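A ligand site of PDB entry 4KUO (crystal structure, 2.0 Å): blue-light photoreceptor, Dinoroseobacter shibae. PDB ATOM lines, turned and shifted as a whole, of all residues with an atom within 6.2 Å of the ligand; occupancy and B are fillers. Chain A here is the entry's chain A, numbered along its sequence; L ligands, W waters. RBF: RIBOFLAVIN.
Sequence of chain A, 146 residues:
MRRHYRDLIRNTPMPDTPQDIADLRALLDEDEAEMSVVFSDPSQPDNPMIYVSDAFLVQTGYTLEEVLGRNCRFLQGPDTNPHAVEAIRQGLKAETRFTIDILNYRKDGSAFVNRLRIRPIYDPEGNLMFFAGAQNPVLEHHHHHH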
ATOM      1  N   VAL A  38      12.558  16.759 -21.551  1.00  0.00           N
ATOM      2  CA  VAL A  38      12.846  15.396 -21.987  1.00  0.00           C
ATOM      3  C   VAL A  38      11.550  14.699 -22.433  1.00  0.00           C
ATOM      4  O   VAL A  38      10.515  14.870 -21.793  1.00  0.00           O
ATOM      5  CB  VAL A  38      13.484  14.585 -20.835  1.00  0.00           C
ATOM      6  CG1 VAL A  38      13.387  13.097 -21.081  1.00  0.00           C
ATOM      7  CG2 VAL A  38      14.919  15.019 -20.609  1.00  0.00           C
ATOM      8  N   PHE A  39      11.618  13.908 -23.510  1.00  0.00           N
ATOM      9  CA  PHE A  39      10.490  13.054 -23.901  1.00  0.00           C
ATOM     10  C   PHE A  39      10.962  11.607 -23.907  1.00  0.00           C
ATOM     11  O   PHE A  39      12.045  11.313 -24.417  1.00  0.00           O
ATOM     12  CB  PHE A  39       9.949  13.423 -25.279  1.00  0.00           C
ATOM     13  CG  PHE A  39       9.268  14.755 -25.336  1.00  0.00           C
ATOM     14  CD1 PHE A  39       7.970  14.904 -24.879  1.00  0.00           C
ATOM     15  CD2 PHE A  39       9.908  15.853 -25.873  1.00  0.00           C
ATOM     16  CE1 PHE A  39       7.336  16.130 -24.931  1.00  0.00           C
ATOM     17  CE2 PHE A  39       9.274  17.088 -25.926  1.00  0.00           C
ATOM     18  CZ  PHE A  39       7.991  17.220 -25.461  1.00  0.00           C
ATOM     19  N   SER A  40      10.150  10.709 -23.356  1.00  0.00           N
ATOM     20  CA  SER A  40      10.474   9.291 -23.350  1.00  0.00           C
ATOM     21  C   SER A  40       9.385   8.483 -24.057  1.00  0.00           C
ATOM     22  O   SER A  40       8.250   8.945 -24.197  1.00  0.00           O
ATOM     23  CB  SER A  40      10.628   8.771 -21.918  1.00  0.00           C
ATOM     24  OG  SER A  40       9.368   8.486 -21.342  1.00  0.00           O
ATOM     25  N   ASN A  47      11.777   2.282 -21.468  1.00  0.00           N
ATOM     26  CA  ASN A  47      11.253   3.653 -21.511  1.00  0.00           C
ATOM     27  C   ASN A  47      12.346   4.700 -21.805  1.00  0.00           C
ATOM     28  O   ASN A  47      12.620   5.563 -20.967  1.00  0.00           O
ATOM     29  CB  ASN A  47      10.539   3.976 -20.186  1.00  0.00           C
ATOM     30  CG  ASN A  47       9.786   5.293 -20.231  1.00  0.00           C
ATOM     31  OD1 ASN A  47       9.341   5.744 -21.280  1.00  0.00           O
ATOM     32  ND2 ASN A  47       9.636   5.928 -19.073  1.00  0.00           N
ATOM     33  N   MET A  49      14.734   7.754 -23.478  1.00  0.00           N
ATOM     34  CA  MET A  49      14.567   9.119 -23.959  1.00  0.00           C
ATOM     35  C   MET A  49      14.678   9.167 -25.482  1.00  0.00           C
ATOM     36  O   MET A  49      15.608   8.579 -26.059  1.00  0.00           O
ATOM     37  CB  MET A  49      15.613  10.031 -23.325  1.00  0.00           C
ATOM     38  CG  MET A  49      15.348  10.302 -21.867  1.00  0.00           C
ATOM     39  SD  MET A  49      16.778  11.047 -21.078  1.00  0.00           S
ATOM     40  CE  MET A  49      17.902   9.688 -21.235  1.00  0.00           C
ATOM     41  N   PHE A  56      19.013  20.620 -21.198  1.00  0.00           N
ATOM     42  CA  PHE A  56      19.193  19.379 -20.452  1.00  0.00           C
ATOM     43  C   PHE A  56      20.631  18.899 -20.569  1.00  0.00           C
ATOM     44  O   PHE A  56      21.267  18.548 -19.579  1.00  0.00           O
ATOM     45  CB  PHE A  56      18.237  18.295 -20.962  1.00  0.00           C
ATOM     46  CG  PHE A  56      18.412  16.959 -20.281  1.00  0.00           C
ATOM     47  CD1 PHE A  56      17.702  16.646 -19.131  1.00  0.00           C
ATOM     48  CD2 PHE A  56      19.272  16.005 -20.809  1.00  0.00           C
ATOM     49  CE1 PHE A  56      17.851  15.419 -18.509  1.00  0.00           C
ATOM     50  CE2 PHE A  56      19.431  14.768 -20.188  1.00  0.00           C
ATOM     51  CZ  PHE A  56      18.722  14.476 -19.034  1.00  0.00           C
ATOM     52  N   ASN A  71      17.512   5.191 -20.578  1.00  0.00           N
ATOM     53  CA  ASN A  71      16.553   5.634 -19.567  1.00  0.00           C
ATOM     54  C   ASN A  71      17.173   6.763 -18.748  1.00  0.00           C
ATOM     55  O   ASN A  71      18.368   6.742 -18.470  1.00  0.00           O
ATOM     56  CB  ASN A  71      16.140   4.472 -18.678  1.00  0.00           C
ATOM     57  CG  ASN A  71      15.038   4.843 -17.701  1.00  0.00           C
ATOM     58  OD1 ASN A  71      15.295   5.446 -16.662  1.00  0.00           O
ATOM     59  ND2 ASN A  71      13.809   4.463 -18.026  1.00  0.00           N
ATOM     60  N   CYS A  72      16.359   7.730 -18.342  1.00  0.00           N
ATOM     61  CA  CYS A  72      16.881   8.922 -17.674  1.00  0.00           C
ATOM     62  C   CYS A  72      17.422   8.652 -16.263  1.00  0.00           C
ATOM     63  O   CYS A  72      17.897   9.575 -15.590  1.00  0.00           O
ATOM     64  CB  CYS A  72      15.805  10.020 -17.620  1.00  0.00           C
ATOM     65  SG  CYS A  72      16.467  11.709 -17.594  1.00  0.00           S
ATOM     66  N   ARG A  73      17.385   7.402 -15.823  1.00  0.00           N
ATOM     67  CA  ARG A  73      17.901   7.041 -14.502  1.00  0.00           C
ATOM     68  C   ARG A  73      19.424   7.160 -14.417  1.00  0.00           C
ATOM     69  O   ARG A  73      19.999   7.026 -13.330  1.00  0.00           O
ATOM     70  CB  ARG A  73      17.444   5.642 -14.084  1.00  0.00           C
ATOM     71  CG  ARG A  73      18.058   4.518 -14.891  1.00  0.00           C
ATOM     72  CD  ARG A  73      17.655   3.164 -14.317  1.00  0.00           C
ATOM     73  NE  ARG A  73      16.204   3.063 -14.181  1.00  0.00           N
ATOM     74  CZ  ARG A  73      15.406   2.587 -15.132  1.00  0.00           C
ATOM     75  NH1 ARG A  73      15.914   2.164 -16.281  1.00  0.00           N
ATOM     76  NH2 ARG A  73      14.094   2.535 -14.922  1.00  0.00           N
ATOM     77  N   LEU A  75      20.896   9.741 -14.540  1.00  0.00           N
ATOM     78  CA  LEU A  75      21.103  10.947 -13.743  1.00  0.00           C
ATOM     79  C   LEU A  75      21.148  10.643 -12.248  1.00  0.00           C
ATOM     80  O   LEU A  75      21.568  11.471 -11.453  1.00  0.00           O
ATOM     81  CB  LEU A  75      19.994  11.978 -14.026  1.00  0.00           C
ATOM     82  CG  LEU A  75      20.020  12.663 -15.385  1.00  0.00           C
ATOM     83  CD1 LEU A  75      19.037  13.825 -15.418  1.00  0.00           C
ATOM     84  CD2 LEU A  75      21.432  13.140 -15.724  1.00  0.00           C
ATOM     85  N   GLN A  76      20.702   9.452 -11.872  1.00  0.00           N
ATOM     86  CA  GLN A  76      20.698   9.063 -10.470  1.00  0.00           C
ATOM     87  C   GLN A  76      22.089   8.591 -10.036  1.00  0.00           C
ATOM     88  O   GLN A  76      22.860   8.084 -10.853  1.00  0.00           O
ATOM     89  CB  GLN A  76      19.632   8.001 -10.217  1.00  0.00           C
ATOM     90  CG  GLN A  76      18.221   8.547 -10.415  1.00  0.00           C
ATOM     91  CD  GLN A  76      17.203   7.467 -10.711  1.00  0.00           C
ATOM     92  OE1 GLN A  76      17.459   6.275 -10.497  1.00  0.00           O
ATOM     93  NE2 GLN A  76      16.040   7.869 -11.202  1.00  0.00           N
ATOM     94  N   THR A  80      21.278   9.256  -4.177  1.00  0.00           N
ATOM     95  CA  THR A  80      19.897   9.402  -4.606  1.00  0.00           C
ATOM     96  C   THR A  80      18.999   8.514  -3.743  1.00  0.00           C
ATOM     97  O   THR A  80      19.313   7.355  -3.495  1.00  0.00           O
ATOM     98  CB  THR A  80      19.720   9.021  -6.085  1.00  0.00           C
ATOM     99  OG1 THR A  80      20.528   9.878  -6.903  1.00  0.00           O
ATOM    100  CG2 THR A  80      18.253   9.160  -6.509  1.00  0.00           C
ATOM    101  N   VAL A  85      13.012   7.221  -6.168  1.00  0.00           N
ATOM    102  CA  VAL A  85      13.060   6.503  -7.442  1.00  0.00           C
ATOM    103  C   VAL A  85      11.812   5.656  -7.629  1.00  0.00           C
ATOM    104  O   VAL A  85      11.213   5.636  -8.703  1.00  0.00           O
ATOM    105  CB  VAL A  85      14.317   5.619  -7.544  1.00  0.00           C
ATOM    106  CG1 VAL A  85      14.264   4.749  -8.806  1.00  0.00           C
ATOM    107  CG2 VAL A  85      15.583   6.473  -7.544  1.00  0.00           C
ATOM    108  N   GLU A  86      11.416   4.956  -6.577  1.00  0.00           N
ATOM    109  CA  GLU A  86      10.231   4.098  -6.643  1.00  0.00           C
ATOM    110  C   GLU A  86       8.938   4.923  -6.779  1.00  0.00           C
ATOM    111  O   GLU A  86       7.992   4.507  -7.438  1.00  0.00           O
ATOM    112  CB  GLU A  86      10.155   3.153  -5.437  1.00  0.00           C
ATOM    113  CG  GLU A  86       8.970   2.191  -5.457  1.00  0.00           C
ATOM    114  CD  GLU A  86       8.949   1.308  -6.696  1.00  0.00           C
ATOM    115  OE1 GLU A  86      10.018   0.986  -7.238  1.00  0.00           O
ATOM    116  OE2 GLU A  86       7.838   0.930  -7.127  1.00  0.00           O
ATOM    117  N   ILE A  88       8.682   7.725  -8.422  1.00  0.00           N
ATOM    118  CA  ILE A  88       8.605   8.072  -9.836  1.00  0.00           C
ATOM    119  C   ILE A  88       8.065   6.917 -10.672  1.00  0.00           C
ATOM    120  O   ILE A  88       7.206   7.107 -11.530  1.00  0.00           O
ATOM    121  CB  ILE A  88       9.984   8.486 -10.381  1.00  0.00           C
ATOM    122  CG1 ILE A  88      10.482   9.747  -9.664  1.00  0.00           C
ATOM    123  CG2 ILE A  88       9.911   8.723 -11.893  1.00  0.00           C
ATOM    124  CD1 ILE A  88      11.913  10.133 -10.013  1.00  0.00           C
ATOM    125  N   ARG A  89       8.573   5.710 -10.405  1.00  0.00           N
ATOM    126  CA  ARG A  89       8.163   4.525 -11.143  1.00  0.00           C
ATOM    127  C   ARG A  89       6.653   4.304 -11.022  1.00  0.00           C
ATOM    128  O   ARG A  89       5.974   4.036 -12.016  1.00  0.00           O
ATOM    129  CB  ARG A  89       8.927   3.294 -10.657  1.00  0.00           C
ATOM    130  CG  ARG A  89       8.764   2.073 -11.558  1.00  0.00           C
ATOM    131  CD  ARG A  89       9.575   0.893 -11.037  1.00  0.00           C
ATOM    132  NE  ARG A  89       8.917   0.244  -9.909  1.00  0.00           N
ATOM    133  CZ  ARG A  89       8.199  -0.872 -10.012  1.00  0.00           C
ATOM    134  NH1 ARG A  89       8.056  -1.458 -11.192  1.00  0.00           N
ATOM    135  NH2 ARG A  89       7.637  -1.398  -8.931  1.00  0.00           N
ATOM    136  N   LEU A  92       4.618   6.964 -12.892  1.00  0.00           N
ATOM    137  CA  LEU A  92       4.552   6.646 -14.311  1.00  0.00           C
ATOM    138  C   LEU A  92       3.455   5.624 -14.587  1.00  0.00           C
ATOM    139  O   LEU A  92       2.661   5.785 -15.522  1.00  0.00           O
ATOM    140  CB  LEU A  92       5.906   6.127 -14.805  1.00  0.00           C
ATOM    141  CG  LEU A  92       7.057   7.132 -14.814  1.00  0.00           C
ATOM    142  CD1 LEU A  92       8.349   6.462 -15.258  1.00  0.00           C
ATOM    143  CD2 LEU A  92       6.731   8.332 -15.700  1.00  0.00           C
ATOM    144  N   ILE A 102      14.443  15.244  -6.487  1.00  0.00           N
ATOM    145  CA  ILE A 102      15.308  14.069  -6.400  1.00  0.00           C
ATOM    146  C   ILE A 102      16.764  14.468  -6.641  1.00  0.00           C
ATOM    147  O   ILE A 102      17.064  15.321  -7.477  1.00  0.00           O
ATOM    148  CB  ILE A 102      14.856  12.982  -7.411  1.00  0.00           C
ATOM    149  CG1 ILE A 102      15.666  11.703  -7.254  1.00  0.00           C
ATOM    150  CG2 ILE A 102      14.919  13.503  -8.846  1.00  0.00           C
ATOM    151  CD1 ILE A 102      15.100  10.532  -8.052  1.00  0.00           C
ATOM    152  N   LEU A 103      17.672  13.878  -5.865  1.00  0.00           N
ATOM    153  CA  LEU A 103      19.094  14.174  -6.034  1.00  0.00           C
ATOM    154  C   LEU A 103      19.609  13.561  -7.329  1.00  0.00           C
ATOM    155  O   LEU A 103      19.569  12.346  -7.506  1.00  0.00           O
ATOM    156  CB  LEU A 103      19.897  13.676  -4.836  1.00  0.00           C
ATOM    157  CG  LEU A 103      21.373  14.088  -4.799  1.00  0.00           C
ATOM    158  CD1 LEU A 103      21.499  15.600  -4.660  1.00  0.00           C
ATOM    159  CD2 LEU A 103      22.104  13.383  -3.677  1.00  0.00           C
ATOM    160  N   ASN A 104      20.089  14.410  -8.229  1.00  0.00           N
ATOM    161  CA  ASN A 104      20.658  13.941  -9.491  1.00  0.00           C
ATOM    162  C   ASN A 104      22.121  14.342  -9.613  1.00  0.00           C
ATOM    163  O   ASN A 104      22.611  15.154  -8.832  1.00  0.00           O
ATOM    164  CB  ASN A 104      19.885  14.493 -10.693  1.00  0.00           C
ATOM    165  CG  ASN A 104      18.631  13.690 -11.020  1.00  0.00           C
ATOM    166  OD1 ASN A 104      17.847  14.093 -11.871  1.00  0.00           O
ATOM    167  ND2 ASN A 104      18.432  12.562 -10.341  1.00  0.00           N
ATOM    168  N   ASN A 114      17.128  18.092  -8.216  1.00  0.00           N
ATOM    169  CA  ASN A 114      16.372  18.262  -9.446  1.00  0.00           C
ATOM    170  C   ASN A 114      14.866  18.232  -9.181  1.00  0.00           C
ATOM    171  O   ASN A 114      14.344  17.244  -8.665  1.00  0.00           O
ATOM    172  CB  ASN A 114      16.759  17.153 -10.427  1.00  0.00           C
ATOM    173  CG  ASN A 114      16.312  17.431 -11.846  1.00  0.00           C
ATOM    174  OD1 ASN A 114      15.970  18.559 -12.187  1.00  0.00           O
ATOM    175  ND2 ASN A 114      16.316  16.404 -12.675  1.00  0.00           N
ATOM    176  N   LEU A 116      11.671  17.576 -10.712  1.00  0.00           N
ATOM    177  CA  LEU A 116      11.237  16.857 -11.893  1.00  0.00           C
ATOM    178  C   LEU A 116       9.727  16.916 -12.014  1.00  0.00           C
ATOM    179  O   LEU A 116       9.011  16.550 -11.084  1.00  0.00           O
ATOM    180  CB  LEU A 116      11.712  15.405 -11.766  1.00  0.00           C
ATOM    181  CG  LEU A 116      11.338  14.359 -12.819  1.00  0.00           C
ATOM    182  CD1 LEU A 116      11.751  14.823 -14.200  1.00  0.00           C
ATOM    183  CD2 LEU A 116      12.010  13.044 -12.452  1.00  0.00           C
ATOM    184  N   ILE A 118       6.611  15.555 -14.391  1.00  0.00           N
ATOM    185  CA  ILE A 118       6.320  14.572 -15.426  1.00  0.00           C
ATOM    186  C   ILE A 118       4.820  14.499 -15.709  1.00  0.00           C
ATOM    187  O   ILE A 118       4.001  14.580 -14.795  1.00  0.00           O
ATOM    188  CB  ILE A 118       6.859  13.180 -15.018  1.00  0.00           C
ATOM    189  CG1 ILE A 118       8.388  13.225 -14.897  1.00  0.00           C
ATOM    190  CG2 ILE A 118       6.441  12.107 -16.024  1.00  0.00           C
ATOM    191  CD1 ILE A 118       9.024  11.920 -14.461  1.00  0.00           C
ATOM    192  N   PHE A 131       5.949  10.129 -22.449  1.00  0.00           N
ATOM    193  CA  PHE A 131       6.001  10.901 -21.218  1.00  0.00           C
ATOM    194  C   PHE A 131       6.800  12.165 -21.505  1.00  0.00           C
ATOM    195  O   PHE A 131       7.794  12.116 -22.235  1.00  0.00           O
ATOM    196  CB  PHE A 131       6.664  10.120 -20.084  1.00  0.00           C
ATOM    197  CG  PHE A 131       5.774   9.109 -19.440  1.00  0.00           C
ATOM    198  CD1 PHE A 131       4.718   9.503 -18.632  1.00  0.00           C
ATOM    199  CD2 PHE A 131       5.993   7.755 -19.627  1.00  0.00           C
ATOM    200  CE1 PHE A 131       3.894   8.572 -18.034  1.00  0.00           C
ATOM    201  CE2 PHE A 131       5.169   6.814 -19.028  1.00  0.00           C
ATOM    202  CZ  PHE A 131       4.121   7.228 -18.227  1.00  0.00           C
ATOM    203  N   ALA A 132       6.366  13.282 -20.939  1.00  0.00           N
ATOM    204  CA  ALA A 132       7.108  14.522 -21.053  1.00  0.00           C
ATOM    205  C   ALA A 132       7.628  14.916 -19.687  1.00  0.00           C
ATOM    206  O   ALA A 132       6.899  14.837 -18.696  1.00  0.00           O
ATOM    207  CB  ALA A 132       6.226  15.625 -21.615  1.00  0.00           C
ATOM    208  N   GLY A 133       8.886  15.322 -19.624  1.00  0.00           N
ATOM    209  CA  GLY A 133       9.496  15.723 -18.377  1.00  0.00           C
ATOM    210  C   GLY A 133      10.119  17.106 -18.484  1.00  0.00           C
ATOM    211  O   GLY A 133      10.793  17.418 -19.462  1.00  0.00           O
ATOM    212  N   ALA A 134       9.866  17.936 -17.483  1.00  0.00           N
ATOM    213  CA  ALA A 134      10.491  19.241 -17.407  1.00  0.00           C
ATOM    214  C   ALA A 134      11.274  19.323 -16.102  1.00  0.00           C
ATOM    215  O   ALA A 134      10.724  19.103 -15.031  1.00  0.00           O
ATOM    216  CB  ALA A 134       9.448  20.349 -17.480  1.00  0.00           C
ATOM    217  N   GLN A 135      12.573  19.599 -16.203  1.00  0.00           N
ATOM    218  CA  GLN A 135      13.433  19.623 -15.028  1.00  0.00           C
ATOM    219  C   GLN A 135      14.027  21.002 -14.768  1.00  0.00           C
ATOM    220  O   GLN A 135      14.217  21.797 -15.688  1.00  0.00           O
ATOM    221  CB  GLN A 135      14.583  18.626 -15.181  1.00  0.00           C
ATOM    222  CG  GLN A 135      14.142  17.186 -15.315  1.00  0.00           C
ATOM    223  CD  GLN A 135      14.325  16.660 -16.723  1.00  0.00           C
ATOM    224  OE1 GLN A 135      14.718  17.397 -17.627  1.00  0.00           O
ATOM    225  NE2 GLN A 135      14.054  15.380 -16.910  1.00  0.00           N
HETATM  226  N1  RBF L   1      14.823  10.528 -13.140  1.00  0.00           N
HETATM  227  C2  RBF L   1      15.778  11.358 -12.671  1.00  0.00           C
HETATM  228  O2  RBF L   1      16.447  10.991 -11.680  1.00  0.00           O
HETATM  229  N3  RBF L   1      16.042  12.570 -13.220  1.00  0.00           N
HETATM  230  C4  RBF L   1      15.375  13.027 -14.277  1.00  0.00           C
HETATM  231  O4  RBF L   1      15.629  14.144 -14.778  1.00  0.00           O
HETATM  232  C4A RBF L   1      14.307  12.174 -14.860  1.00  0.00           C
HETATM  233  N5  RBF L   1      13.585  12.564 -15.923  1.00  0.00           N
HETATM  234  C5A RBF L   1      12.604  11.775 -16.425  1.00  0.00           C
HETATM  235  C6  RBF L   1      11.866  12.208 -17.524  1.00  0.00           C
HETATM  236  C7  RBF L   1      10.866  11.409 -18.071  1.00  0.00           C
HETATM  237  C7M RBF L   1      10.087  11.891 -19.264  1.00  0.00           C
HETATM  238  C8  RBF L   1      10.576  10.084 -17.462  1.00  0.00           C
HETATM  239  C8M RBF L   1       9.497   9.209 -18.047  1.00  0.00           C
HETATM  240  C9  RBF L   1      11.315   9.642 -16.361  1.00  0.00           C
HETATM  241  C9A RBF L   1      12.311  10.438 -15.823  1.00  0.00           C
HETATM  242  N10 RBF L   1      13.066  10.010 -14.710  1.00  0.00           N
HETATM  243  C10 RBF L   1      14.067  10.862 -14.209  1.00  0.00           C
HETATM  244  C1' RBF L   1      12.805   8.727 -14.057  1.00  0.00           C
HETATM  245  C2' RBF L   1      13.601   7.545 -14.617  1.00  0.00           C
HETATM  246  O2' RBF L   1      13.666   7.598 -16.044  1.00  0.00           O
HETATM  247  C3' RBF L   1      12.904   6.271 -14.170  1.00  0.00           C
HETATM  248  O3' RBF L   1      11.569   6.244 -14.678  1.00  0.00           O
HETATM  249  C4' RBF L   1      12.849   6.208 -12.645  1.00  0.00           C
HETATM  250  O4' RBF L   1      14.173   6.017 -12.149  1.00  0.00           O
HETATM  251  C5' RBF L   1      11.949   5.074 -12.157  1.00  0.00           C
HETATM  252  O5' RBF L   1      12.379   3.825 -12.713  1.00  0.00           O
HETATM  253  O   HOH W   1      13.551   7.527 -19.097  1.00  0.00           O
HETATM  254  O   HOH W   2      15.669   4.119 -11.738  1.00  0.00           O
HETATM  255  O   HOH W   3      13.111   1.811 -10.732  1.00  0.00           O
HETATM  256  O   HOH W   4      11.004   4.634 -16.817  1.00  0.00           O
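The side-chain amide oxygen (OD1) of Asn 104 lies within hydrogen-bond range of a nitrogen (N3) of the ligand (2.7 Å). O2' of the ligand sits at hydrogen-bond distance from OD1 of Asn 71 (2.8 Å). O4' of the ligand lies within hydrogen-bond range of NE2 of Gln 76, 2.8 Å away. The side-chain amide nitrogen (NE2) of Gln 135 sits at hydrogen-bond distance from an oxygen (O4) of the ligand (2.9 Å). NH2 of Arg 73 sits at hydrogen-bond distance from O5' of the ligand (3.1 Å). O4 of the ligand is in hydrogen-bond range of ND2 of Asn 114, at 3.2 Å. A nitrogen (N5) of the ligand lies within hydrogen-bond range of the side-chain sulfur of Cys 72 (3.4 Å).
The side-chain amide oxygen of Asn 104 is in hydrogen-bond range of the side-chain amide nitrogen of Asn 114. OD1 of Asn 71 lies within hydrogen-bond range of N of Arg 73, at 3.0 Å. The backbone NH (N) of Asn 114 sits at hydrogen-bond distance from the backbone carbonyl oxygen (O) of Ile 102 (2.9 Å). OG of Ser 40 is in hydrogen-bond range of OD1 of Asn 47 (2.7 Å). N of Ser 40 sits at hydrogen-bond distance from O of Phe 131, at 3.0 Å. The side-chain sulfur of Met 49 sits at hydrogen-bond distance from the side-chain sulfur of Cys 72 (3.6 Å). The backbone NH (N) of Gly 133 lies within hydrogen-bond range of the backbone carbonyl oxygen (O) of Val 38. NH2 of Arg 89 lies within salt-bridge range of OE2 of Glu 86, 3.0 Å away.
Val 38 touches the ligand. Ser 40 touches the ligand. Asn 47 touches the ligand. Leu 75 touches the ligand (CD1 to O4, 3.5 Å). Val 85 touches the ligand. Ile 88 touches the ligand. CB of Arg 89 touches C5' of the ligand (3.8 Å). Leu 92 touches the ligand (CD1 to O3', 3.3 Å). CD1 of Ile 102 touches O2 of the ligand, 3.9 Å away. CD1 of Leu 116 touches N5 of the ligand, 3.4 Å away. Ile 118 touches the ligand. CB of Phe 131 touches C8M of the ligand (3.6 Å). Ala 132 touches the ligand (C to C7M, 3.9 Å). N of Gly 133 touches C7M of the ligand, 3.7 Å away. Of the 28 residues printed, 21 come within 4 Å of the ligand. Along chain A the residues within 4 Å of the ligand span positions 38 to 135. The nearest printed residue that does not touch the ligand is Phe 56 (4.5 Å).
Water W2 lies within hydrogen-bond range of an oxygen (O4') of the ligand (2.5 Å), the guanidinium group (NE) of Arg 73 (2.7 Å) and the side-chain amide oxygen (OE1) of Gln 76 (3.1 Å). Water W4 lies within hydrogen-bond range of O3' of the ligand, ND2 of Asn 47 and ND2 of Asn 71. Water W1 lies within hydrogen-bond range of O of Asn 47, N of Cys 72, O2' of the ligand and ND2 of Asn 71.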
